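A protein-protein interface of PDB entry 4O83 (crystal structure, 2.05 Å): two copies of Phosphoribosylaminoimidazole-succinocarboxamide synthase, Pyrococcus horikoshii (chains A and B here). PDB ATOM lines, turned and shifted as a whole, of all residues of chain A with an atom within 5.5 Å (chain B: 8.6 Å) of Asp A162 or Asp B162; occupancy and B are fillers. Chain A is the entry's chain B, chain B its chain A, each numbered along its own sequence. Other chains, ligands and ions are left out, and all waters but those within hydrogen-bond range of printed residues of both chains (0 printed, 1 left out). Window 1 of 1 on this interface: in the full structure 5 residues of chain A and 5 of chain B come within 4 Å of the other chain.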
ATOM      1  N   ASN A 157      -7.017 -17.420 -20.939  1.00  0.00           N
ATOM      2  CA  ASN A 157      -6.649 -16.899 -22.249  1.00  0.00           C
ATOM      3  C   ASN A 157      -7.588 -15.805 -22.751  1.00  0.00           C
ATOM      4  O   ASN A 157      -7.146 -14.734 -23.146  1.00  0.00           O
ATOM      5  CB  ASN A 157      -6.569 -18.020 -23.289  1.00  0.00           C
ATOM      6  CG  ASN A 157      -6.069 -17.529 -24.639  1.00  0.00           C
ATOM      7  OD1 ASN A 157      -4.948 -17.029 -24.752  1.00  0.00           O
ATOM      8  ND2 ASN A 157      -6.886 -17.689 -25.670  1.00  0.00           N
ATOM      9  N   GLU A 158      -8.886 -16.071 -22.735  1.00  0.00           N
ATOM     10  CA  GLU A 158      -9.808 -15.107 -23.313  1.00  0.00           C
ATOM     11  C   GLU A 158      -9.801 -13.757 -22.573  1.00  0.00           C
ATOM     12  O   GLU A 158      -9.791 -12.696 -23.212  1.00  0.00           O
ATOM     13  CB  GLU A 158     -11.226 -15.664 -23.428  1.00  0.00           C
ATOM     14  CG  GLU A 158     -11.979 -15.043 -24.612  1.00  0.00           C
ATOM     15  CD  GLU A 158     -11.325 -15.337 -25.972  1.00  0.00           C
ATOM     16  OE1 GLU A 158     -10.611 -16.363 -26.132  1.00  0.00           O
ATOM     17  OE2 GLU A 158     -11.532 -14.558 -26.913  1.00  0.00           O
ATOM     18  N   ILE A 159      -9.785 -13.824 -21.246  1.00  0.00           N
ATOM     19  CA  ILE A 159      -9.717 -12.639 -20.374  1.00  0.00           C
ATOM     20  C   ILE A 159      -8.417 -11.840 -20.560  1.00  0.00           C
ATOM     21  O   ILE A 159      -8.457 -10.620 -20.764  1.00  0.00           O
ATOM     22  CB  ILE A 159      -9.871 -13.029 -18.876  1.00  0.00           C
ATOM     23  CG1 ILE A 159     -11.248 -13.670 -18.621  1.00  0.00           C
ATOM     24  CG2 ILE A 159      -9.625 -11.819 -17.965  1.00  0.00           C
ATOM     25  CD1 ILE A 159     -11.354 -14.454 -17.317  1.00  0.00           C
ATOM     26  N   LEU A 160      -7.278 -12.517 -20.458  1.00  0.00           N
ATOM     27  CA  LEU A 160      -5.993 -11.890 -20.695  1.00  0.00           C
ATOM     28  C   LEU A 160      -5.897 -11.269 -22.095  1.00  0.00           C
ATOM     29  O   LEU A 160      -5.555 -10.087 -22.224  1.00  0.00           O
ATOM     30  CB  LEU A 160      -4.839 -12.870 -20.398  1.00  0.00           C
ATOM     31  CG  LEU A 160      -4.660 -13.359 -18.943  1.00  0.00           C
ATOM     32  CD1 LEU A 160      -3.393 -14.167 -18.752  1.00  0.00           C
ATOM     33  CD2 LEU A 160      -4.671 -12.216 -17.921  1.00  0.00           C
ATOM     34  N   LYS A 161      -6.258 -12.035 -23.124  1.00  0.00           N
ATOM     35  CA  LYS A 161      -6.178 -11.586 -24.509  1.00  0.00           C
ATOM     36  C   LYS A 161      -7.019 -10.340 -24.764  1.00  0.00           C
ATOM     37  O   LYS A 161      -6.556  -9.383 -25.402  1.00  0.00           O
ATOM     38  CB  LYS A 161      -6.571 -12.696 -25.488  1.00  0.00           C
ATOM     39  CG  LYS A 161      -6.581 -12.240 -26.940  1.00  0.00           C
ATOM     40  CD  LYS A 161      -7.221 -13.226 -27.896  1.00  0.00           C
ATOM     41  CE  LYS A 161      -8.667 -13.483 -27.536  1.00  0.00           C
ATOM     42  NZ  LYS A 161      -9.403 -14.179 -28.628  1.00  0.00           N
ATOM     43  N   ASP A 162      -8.243 -10.349 -24.248  1.00  0.00           N
ATOM     44  CA  ASP A 162      -9.145  -9.233 -24.480  1.00  0.00           C
ATOM     45  C   ASP A 162      -8.681  -7.980 -23.755  1.00  0.00           C
ATOM     46  O   ASP A 162      -8.722  -6.889 -24.330  1.00  0.00           O
ATOM     47  CB  ASP A 162     -10.589  -9.607 -24.127  1.00  0.00           C
ATOM     48  CG  ASP A 162     -11.149 -10.718 -25.016  1.00  0.00           C
ATOM     49  OD1 ASP A 162     -10.534 -11.072 -26.063  1.00  0.00           O
ATOM     50  OD2 ASP A 162     -12.212 -11.266 -24.681  1.00  0.00           O
ATOM     51  N   TYR A 163      -8.234  -8.154 -22.506  1.00  0.00           N
ATOM     52  CA  TYR A 163      -7.725  -7.101 -21.669  1.00  0.00           C
ATOM     53  C   TYR A 163      -6.534  -6.415 -22.348  1.00  0.00           C
ATOM     54  O   TYR A 163      -6.500  -5.187 -22.469  1.00  0.00           O
ATOM     55  CB  TYR A 163      -7.323  -7.677 -20.304  1.00  0.00           C
ATOM     56  CG  TYR A 163      -6.790  -6.671 -19.316  1.00  0.00           C
ATOM     57  CD1 TYR A 163      -7.642  -5.757 -18.690  1.00  0.00           C
ATOM     58  CD2 TYR A 163      -5.437  -6.640 -18.990  1.00  0.00           C
ATOM     59  CE1 TYR A 163      -7.149  -4.828 -17.772  1.00  0.00           C
ATOM     60  CE2 TYR A 163      -4.937  -5.719 -18.077  1.00  0.00           C
ATOM     61  CZ  TYR A 163      -5.793  -4.819 -17.471  1.00  0.00           C
ATOM     62  OH  TYR A 163      -5.293  -3.912 -16.564  1.00  0.00           O
ATOM     63  N   LEU A 164      -5.586  -7.220 -22.824  1.00  0.00           N
ATOM     64  CA  LEU A 164      -4.367  -6.691 -23.412  1.00  0.00           C
ATOM     65  C   LEU A 164      -4.592  -6.076 -24.793  1.00  0.00           C
ATOM     66  O   LEU A 164      -3.936  -5.093 -25.142  1.00  0.00           O
ATOM     67  CB  LEU A 164      -3.262  -7.763 -23.447  1.00  0.00           C
ATOM     68  CG  LEU A 164      -2.821  -8.301 -22.078  1.00  0.00           C
ATOM     69  CD1 LEU A 164      -2.015  -9.604 -22.209  1.00  0.00           C
ATOM     70  CD2 LEU A 164      -2.061  -7.238 -21.294  1.00  0.00           C
ATOM     71  N   ALA A 165      -5.539  -6.629 -25.551  1.00  0.00           N
ATOM     72  CA  ALA A 165      -5.842  -6.140 -26.881  1.00  0.00           C
ATOM     73  C   ALA A 165      -6.321  -4.696 -26.828  1.00  0.00           C
ATOM     74  O   ALA A 165      -5.949  -3.893 -27.677  1.00  0.00           O
ATOM     75  CB  ALA A 165      -6.887  -7.026 -27.561  1.00  0.00           C
ATOM     76  N   LYS A 166      -7.141  -4.372 -25.829  1.00  0.00           N
ATOM     77  CA  LYS A 166      -7.658  -3.010 -25.647  1.00  0.00           C
ATOM     78  C   LYS A 166      -6.529  -2.006 -25.403  1.00  0.00           C
ATOM     79  O   LYS A 166      -6.714  -0.791 -25.533  1.00  0.00           O
ATOM     80  CB  LYS A 166      -8.677  -2.972 -24.506  1.00  0.00           C
ATOM     81  CG  LYS A 166      -9.962  -3.699 -24.839  1.00  0.00           C
ATOM     82  CD  LYS A 166     -10.777  -3.992 -23.587  1.00  0.00           C
ATOM     83  CE  LYS A 166     -11.987  -4.840 -23.931  1.00  0.00           C
ATOM     84  NZ  LYS A 166     -12.582  -5.478 -22.722  1.00  0.00           N
ATOM     85  N   LEU B  59     -14.619 -10.813 -42.559  1.00  0.00           N
ATOM     86  CA  LEU B  59     -13.963 -11.089 -41.296  1.00  0.00           C
ATOM     87  C   LEU B  59     -14.345 -12.475 -40.731  1.00  0.00           C
ATOM     88  O   LEU B  59     -13.473 -13.277 -40.388  1.00  0.00           O
ATOM     89  CB  LEU B  59     -14.286  -9.996 -40.279  1.00  0.00           C
ATOM     90  CG  LEU B  59     -13.647 -10.147 -38.900  1.00  0.00           C
ATOM     91  CD1 LEU B  59     -12.119 -10.060 -38.965  1.00  0.00           C
ATOM     92  CD2 LEU B  59     -14.199  -9.088 -37.949  1.00  0.00           C
ATOM     93  N   HIS B  63     -12.285 -16.505 -40.380  1.00  0.00           N
ATOM     94  CA  HIS B  63     -12.200 -17.369 -39.192  1.00  0.00           C
ATOM     95  C   HIS B  63     -12.865 -18.704 -39.364  1.00  0.00           C
ATOM     96  O   HIS B  63     -12.972 -19.499 -38.409  1.00  0.00           O
ATOM     97  CB  HIS B  63     -12.770 -16.648 -37.982  1.00  0.00           C
ATOM     98  CG  HIS B  63     -11.947 -15.461 -37.550  1.00  0.00           C
ATOM     99  ND1 HIS B  63     -11.876 -14.325 -38.273  1.00  0.00           N
ATOM    100  CD2 HIS B  63     -11.133 -15.276 -36.447  1.00  0.00           C
ATOM    101  CE1 HIS B  63     -11.062 -13.454 -37.656  1.00  0.00           C
ATOM    102  NE2 HIS B  63     -10.619 -14.032 -36.531  1.00  0.00           N
ATOM    103  N   ASN B  94     -23.722  -9.069 -24.694  1.00  0.00           N
ATOM    104  CA  ASN B  94     -22.524  -8.958 -23.862  1.00  0.00           C
ATOM    105  C   ASN B  94     -22.713  -7.996 -22.675  1.00  0.00           C
ATOM    106  O   ASN B  94     -22.061  -8.112 -21.637  1.00  0.00           O
ATOM    107  CB  ASN B  94     -21.361  -8.502 -24.738  1.00  0.00           C
ATOM    108  CG  ASN B  94     -21.025  -9.518 -25.811  1.00  0.00           C
ATOM    109  OD1 ASN B  94     -20.742 -10.674 -25.502  1.00  0.00           O
ATOM    110  ND2 ASN B  94     -21.092  -9.103 -27.081  1.00  0.00           N
ATOM    111  N   LEU B 154     -22.133 -17.786 -30.719  1.00  0.00           N
ATOM    112  CA  LEU B 154     -21.122 -17.442 -29.728  1.00  0.00           C
ATOM    113  C   LEU B 154     -19.726 -17.211 -30.331  1.00  0.00           C
ATOM    114  O   LEU B 154     -19.014 -16.300 -29.927  1.00  0.00           O
ATOM    115  CB  LEU B 154     -21.100 -18.457 -28.569  1.00  0.00           C
ATOM    116  CG  LEU B 154     -22.341 -18.401 -27.646  1.00  0.00           C
ATOM    117  CD1 LEU B 154     -22.548 -19.690 -26.853  1.00  0.00           C
ATOM    118  CD2 LEU B 154     -22.255 -17.214 -26.696  1.00  0.00           C
ATOM    119  N   LYS B 155     -19.347 -18.021 -31.303  1.00  0.00           N
ATOM    120  CA  LYS B 155     -18.104 -17.808 -32.045  1.00  0.00           C
ATOM    121  C   LYS B 155     -18.090 -16.452 -32.764  1.00  0.00           C
ATOM    122  O   LYS B 155     -17.134 -15.669 -32.639  1.00  0.00           O
ATOM    123  CB  LYS B 155     -17.934 -18.905 -33.093  1.00  0.00           C
ATOM    124  CG  LYS B 155     -16.877 -19.920 -32.762  1.00  0.00           C
ATOM    125  CD  LYS B 155     -16.774 -20.956 -33.871  1.00  0.00           C
ATOM    126  N   VAL B 156     -19.165 -16.198 -33.508  1.00  0.00           N
ATOM    127  CA  VAL B 156     -19.376 -14.936 -34.215  1.00  0.00           C
ATOM    128  C   VAL B 156     -19.262 -13.784 -33.218  1.00  0.00           C
ATOM    129  O   VAL B 156     -18.487 -12.854 -33.446  1.00  0.00           O
ATOM    130  CB  VAL B 156     -20.718 -14.928 -34.973  1.00  0.00           C
ATOM    131  CG1 VAL B 156     -21.101 -13.527 -35.403  1.00  0.00           C
ATOM    132  CG2 VAL B 156     -20.654 -15.850 -36.183  1.00  0.00           C
ATOM    133  N   ASN B 157     -19.997 -13.875 -32.106  1.00  0.00           N
ATOM    134  CA  ASN B 157     -19.907 -12.878 -31.029  1.00  0.00           C
ATOM    135  C   ASN B 157     -18.469 -12.558 -30.627  1.00  0.00           C
ATOM    136  O   ASN B 157     -18.090 -11.380 -30.559  1.00  0.00           O
ATOM    137  CB  ASN B 157     -20.673 -13.331 -29.780  1.00  0.00           C
ATOM    138  CG  ASN B 157     -20.709 -12.263 -28.697  1.00  0.00           C
ATOM    139  OD1 ASN B 157     -21.211 -11.153 -28.934  1.00  0.00           O
ATOM    140  ND2 ASN B 157     -20.208 -12.595 -27.490  1.00  0.00           N
ATOM    141  N   GLU B 158     -17.679 -13.603 -30.361  1.00  0.00           N
ATOM    142  CA  GLU B 158     -16.349 -13.400 -29.832  1.00  0.00           C
ATOM    143  C   GLU B 158     -15.473 -12.662 -30.849  1.00  0.00           C
ATOM    144  O   GLU B 158     -14.769 -11.721 -30.477  1.00  0.00           O
ATOM    145  CB  GLU B 158     -15.695 -14.696 -29.351  1.00  0.00           C
ATOM    146  CG  GLU B 158     -14.648 -14.484 -28.252  1.00  0.00           C
ATOM    147  CD  GLU B 158     -15.233 -13.886 -26.966  1.00  0.00           C
ATOM    148  OE1 GLU B 158     -16.422 -14.134 -26.660  1.00  0.00           O
ATOM    149  OE2 GLU B 158     -14.504 -13.156 -26.254  1.00  0.00           O
ATOM    150  N   ILE B 159     -15.566 -13.062 -32.118  1.00  0.00           N
ATOM    151  CA  ILE B 159     -14.820 -12.404 -33.224  1.00  0.00           C
ATOM    152  C   ILE B 159     -15.233 -10.938 -33.429  1.00  0.00           C
ATOM    153  O   ILE B 159     -14.389 -10.037 -33.479  1.00  0.00           O
ATOM    154  CB  ILE B 159     -14.949 -13.190 -34.546  1.00  0.00           C
ATOM    155  CG1 ILE B 159     -14.371 -14.607 -34.384  1.00  0.00           C
ATOM    156  CG2 ILE B 159     -14.253 -12.453 -35.694  1.00  0.00           C
ATOM    157  CD1 ILE B 159     -14.900 -15.600 -35.412  1.00  0.00           C
ATOM    158  N   LEU B 160     -16.531 -10.699 -33.520  1.00  0.00           N
ATOM    159  CA  LEU B 160     -17.036  -9.325 -33.667  1.00  0.00           C
ATOM    160  C   LEU B 160     -16.694  -8.448 -32.466  1.00  0.00           C
ATOM    161  O   LEU B 160     -16.188  -7.337 -32.634  1.00  0.00           O
ATOM    162  CB  LEU B 160     -18.540  -9.300 -34.005  1.00  0.00           C
ATOM    163  CG  LEU B 160     -18.984  -9.969 -35.325  1.00  0.00           C
ATOM    164  CD1 LEU B 160     -20.464  -9.780 -35.579  1.00  0.00           C
ATOM    165  CD2 LEU B 160     -18.234  -9.510 -36.567  1.00  0.00           C
ATOM    166  N   LYS B 161     -16.931  -8.957 -31.258  1.00  0.00           N
ATOM    167  CA  LYS B 161     -16.602  -8.233 -30.038  1.00  0.00           C
ATOM    168  C   LYS B 161     -15.137  -7.823 -29.965  1.00  0.00           C
ATOM    169  O   LYS B 161     -14.833  -6.650 -29.664  1.00  0.00           O
ATOM    170  CB  LYS B 161     -16.977  -9.029 -28.778  1.00  0.00           C
ATOM    171  CG  LYS B 161     -16.735  -8.267 -27.479  1.00  0.00           C
ATOM    172  CD  LYS B 161     -16.956  -9.118 -26.227  1.00  0.00           C
ATOM    173  CE  LYS B 161     -16.127 -10.398 -26.304  1.00  0.00           C
ATOM    174  NZ  LYS B 161     -15.937 -11.111 -25.011  1.00  0.00           N
ATOM    175  N   ASP B 162     -14.246  -8.783 -30.216  1.00  0.00           N
ATOM    176  CA  ASP B 162     -12.825  -8.551 -30.080  1.00  0.00           C
ATOM    177  C   ASP B 162     -12.322  -7.576 -31.148  1.00  0.00           C
ATOM    178  O   ASP B 162     -11.557  -6.667 -30.855  1.00  0.00           O
ATOM    179  CB  ASP B 162     -12.074  -9.874 -30.126  1.00  0.00           C
ATOM    180  CG  ASP B 162     -12.379 -10.755 -28.926  1.00  0.00           C
ATOM    181  OD1 ASP B 162     -13.114 -10.282 -28.003  1.00  0.00           O
ATOM    182  OD2 ASP B 162     -11.866 -11.903 -28.895  1.00  0.00           O
ATOM    183  N   TYR B 163     -12.795  -7.763 -32.374  1.00  0.00           N
ATOM    184  CA  TYR B 163     -12.475  -6.877 -33.490  1.00  0.00           C
ATOM    185  C   TYR B 163     -12.847  -5.428 -33.175  1.00  0.00           C
ATOM    186  O   TYR B 163     -12.031  -4.497 -33.332  1.00  0.00           O
ATOM    187  CB  TYR B 163     -13.230  -7.358 -34.729  1.00  0.00           C
ATOM    188  CG  TYR B 163     -12.940  -6.558 -35.986  1.00  0.00           C
ATOM    189  CD1 TYR B 163     -11.703  -6.650 -36.624  1.00  0.00           C
ATOM    190  CD2 TYR B 163     -13.911  -5.741 -36.547  1.00  0.00           C
ATOM    191  CE1 TYR B 163     -11.431  -5.928 -37.782  1.00  0.00           C
ATOM    192  CE2 TYR B 163     -13.653  -5.016 -37.706  1.00  0.00           C
ATOM    193  CZ  TYR B 163     -12.407  -5.120 -38.319  1.00  0.00           C
ATOM    194  OH  TYR B 163     -12.142  -4.394 -39.454  1.00  0.00           O
ATOM    195  N   LEU B 164     -14.074  -5.261 -32.687  1.00  0.00           N
ATOM    196  CA  LEU B 164     -14.635  -3.940 -32.410  1.00  0.00           C
ATOM    197  C   LEU B 164     -14.052  -3.274 -31.171  1.00  0.00           C
ATOM    198  O   LEU B 164     -13.889  -2.048 -31.152  1.00  0.00           O
ATOM    199  CB  LEU B 164     -16.175  -3.987 -32.348  1.00  0.00           C
ATOM    200  CG  LEU B 164     -16.901  -4.367 -33.644  1.00  0.00           C
ATOM    201  CD1 LEU B 164     -18.364  -4.704 -33.329  1.00  0.00           C
ATOM    202  CD2 LEU B 164     -16.799  -3.272 -34.718  1.00  0.00           C
ATOM    203  N   ALA B 165     -13.729  -4.082 -30.157  1.00  0.00           N
ATOM    204  CA  ALA B 165     -13.082  -3.606 -28.924  1.00  0.00           C
ATOM    205  C   ALA B 165     -11.747  -2.918 -29.208  1.00  0.00           C
ATOM    206  O   ALA B 165     -11.436  -1.894 -28.612  1.00  0.00           O
ATOM    207  CB  ALA B 165     -12.876  -4.762 -27.931  1.00  0.00           C
ATOM    208  N   LYS B 166     -10.953  -3.489 -30.114  1.00  0.00           N
ATOM    209  CA  LYS B 166      -9.661  -2.907 -30.485  1.00  0.00           C
ATOM    210  C   LYS B 166      -9.810  -1.529 -31.125  1.00  0.00           C
ATOM    211  O   LYS B 166      -8.847  -0.760 -31.186  1.00  0.00           O
ATOM    212  CB  LYS B 166      -8.897  -3.842 -31.426  1.00  0.00           C
ATOM    213  CG  LYS B 166      -8.426  -5.109 -30.742  1.00  0.00           C
ATOM    214  CD  LYS B 166      -8.048  -6.179 -31.757  1.00  0.00           C
ATOM    215  CE  LYS B 166      -7.820  -7.499 -31.054  1.00  0.00           C
ATOM    216  NZ  LYS B 166      -7.734  -8.614 -32.031  1.00  0.00           N
ATOM    217  N   LYS B 167     -11.028  -1.225 -31.581  1.00  0.00           N
ATOM    218  CA  LYS B 167     -11.345   0.056 -32.231  1.00  0.00           C
ATOM    219  C   LYS B 167     -12.186   0.973 -31.358  1.00  0.00           C
ATOM    220  O   LYS B 167     -12.770   1.945 -31.841  1.00  0.00           O
ATOM    221  CB  LYS B 167     -12.037  -0.205 -33.563  1.00  0.00           C
ATOM    222  CG  LYS B 167     -11.183  -1.051 -34.477  1.00  0.00           C
ATOM    223  CD  LYS B 167     -11.993  -1.577 -35.644  1.00  0.00           C
ATOM    224  CE  LYS B 167     -11.138  -2.503 -36.490  1.00  0.00           C
ATOM    225  NZ  LYS B 167     -10.102  -1.762 -37.257  1.00  0.00           N
ATOM    226  N   GLY B 168     -12.222   0.668 -30.071  1.00  0.00           N
ATOM    227  CA  GLY B 168     -12.943   1.459 -29.076  1.00  0.00           C
ATOM    228  C   GLY B 168     -14.453   1.417 -29.225  1.00  0.00           C
ATOM    229  O   GLY B 168     -15.125   2.387 -28.873  1.00  0.00           O
ATOM    230  N   ILE B 169     -14.977   0.297 -29.745  1.00  0.00           N
ATOM    231  CA  ILE B 169     -16.420   0.053 -29.871  1.00  0.00           C
ATOM    232  C   ILE B 169     -16.862  -1.182 -29.061  1.00  0.00           C
ATOM    233  O   ILE B 169     -16.310  -2.260 -29.232  1.00  0.00           O
ATOM    234  CB  ILE B 169     -16.834  -0.116 -31.353  1.00  0.00           C
ATOM    235  CG1 ILE B 169     -16.504   1.149 -32.161  1.00  0.00           C
ATOM    236  CG2 ILE B 169     -18.329  -0.416 -31.478  1.00  0.00           C
ATOM    237  CD1 ILE B 169     -16.298   0.897 -33.644  1.00  0.00           C
ATOM    238  N   ILE B 170     -17.844  -1.007 -28.171  1.00  0.00           N
ATOM    239  CA  ILE B 170     -18.408  -2.096 -27.398  1.00  0.00           C
ATOM    240  C   ILE B 170     -19.513  -2.769 -28.198  1.00  0.00           C
ATOM    241  O   ILE B 170     -20.497  -2.112 -28.605  1.00  0.00           O
ATOM    242  CB  ILE B 170     -19.054  -1.585 -26.086  1.00  0.00           C
ATOM    243  CG1 ILE B 170     -18.045  -0.823 -25.246  1.00  0.00           C
ATOM    244  CG2 ILE B 170     -19.683  -2.729 -25.273  1.00  0.00           C
ATOM    245  CD1 ILE B 170     -18.715   0.159 -24.296  1.00  0.00           C
ATOM    246  N   LEU B 171     -19.378  -4.074 -28.421  1.00  0.00           N
ATOM    247  CA  LEU B 171     -20.492  -4.823 -28.996  1.00  0.00           C
ATOM    248  C   LEU B 171     -21.462  -5.158 -27.862  1.00  0.00           C
ATOM    249  O   LEU B 171     -21.232  -6.089 -27.075  1.00  0.00           O
ATOM    250  CB  LEU B 171     -20.000  -6.093 -29.691  1.00  0.00           C
ATOM    251  CG  LEU B 171     -21.085  -6.960 -30.349  1.00  0.00           C
ATOM    252  CD1 LEU B 171     -21.791  -6.204 -31.464  1.00  0.00           C
ATOM    253  CD2 LEU B 171     -20.439  -8.225 -30.891  1.00  0.00           C
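OD2 of Asp A162 lies close to NZ of Lys B161, at 3.7 Å. The side-chain carboxylate (OD2) of Asp B162 sits close to the side-chain amino group (NZ) of Lys A161 (3.4 Å). The side-chain carboxylate (OE2) of Glu A158 lies close to the side-chain carboxylate (OE2) of Glu B158 (3.4 Å). The side-chain carboxylate (OD2) of Asp B162 lies close to the side-chain carboxylate (OE2) of Glu A158, 3.3 Å away. The side-chain carboxylate of Asp A162 sits close to the side-chain carboxylate of Glu B158, 3.4 Å away. OD1 of Asp A162 lies close to OD2 of Asp B162 (3.2 Å).
Lys B166 touches Ala A165.
Of the 10 printed residues of chain A, 4 touch a printed residue of chain B. Among the printed residues, 7 pairs touch across the chains. Among the printed residues, Asp or Glu carboxylates within 4 Å of a Lys or Arg side-chain nitrogen of the other chain: Lys A161 with Asp B162 (3.4 Å) and Asp A162 with Lys B161 (3.7 Å).
Glu A158 touches its own counterpart, Glu B158. Glu A158 touches Asp B162, and with the chains exchanged Asp A162 touches Glu B158. Lys A161 touches Asp B162, and with the chains exchanged Asp A162 touches Lys B161. Ala A165 touches Lys B166, but with the chains exchanged Lys A166 does not touch Ala B165 (4.1 Å). Positions printed for both chains: 157, 158, 159, 160, 161, 162, 163, 164, 165 and 166. Of the 7 pairs that touch across the chains among the printed residues, 6 have their exchanged pair printed and touching as well.
Printed residues of chain B within 4 Å of Glu A158: Glu B158 and Asp B162. Of the printed residues of chain B, Lys A161 touches Asp B162 (3.4 Å). Asp A162 touches just these residues of chain B: Glu B158 (3.4 Å), Lys B161 (3.7 Å) and Asp B162 (3.2 Å). Printed residues of chain B within 4 Å of Ala A165: Lys B166 (3.6 Å). Asn B157 touches none of the printed residues of chain A. Of the printed residues of chain A, Glu B158 touches Glu A158 and Asp A162. Of the printed residues of chain A, Lys B161 touches Asp A162 (3.7 Å). Asp B162 touches just these residues of chain A: Glu A158 (3.3 Å), Lys A161 (3.4 Å) and Asp A162 (3.2 Å). Of the printed residues of chain A, Lys B166 touches Ala A165.
The side-chain carboxylate (OE1) of Glu B158 lies within salt-bridge range of the side-chain amino group (NZ) of Lys B161 (3.5 Å). The side-chain carboxylate (OE1) of Glu A158 lies within salt-bridge range of the side-chain amino group (NZ) of Lys A161, at 3.5 Å.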
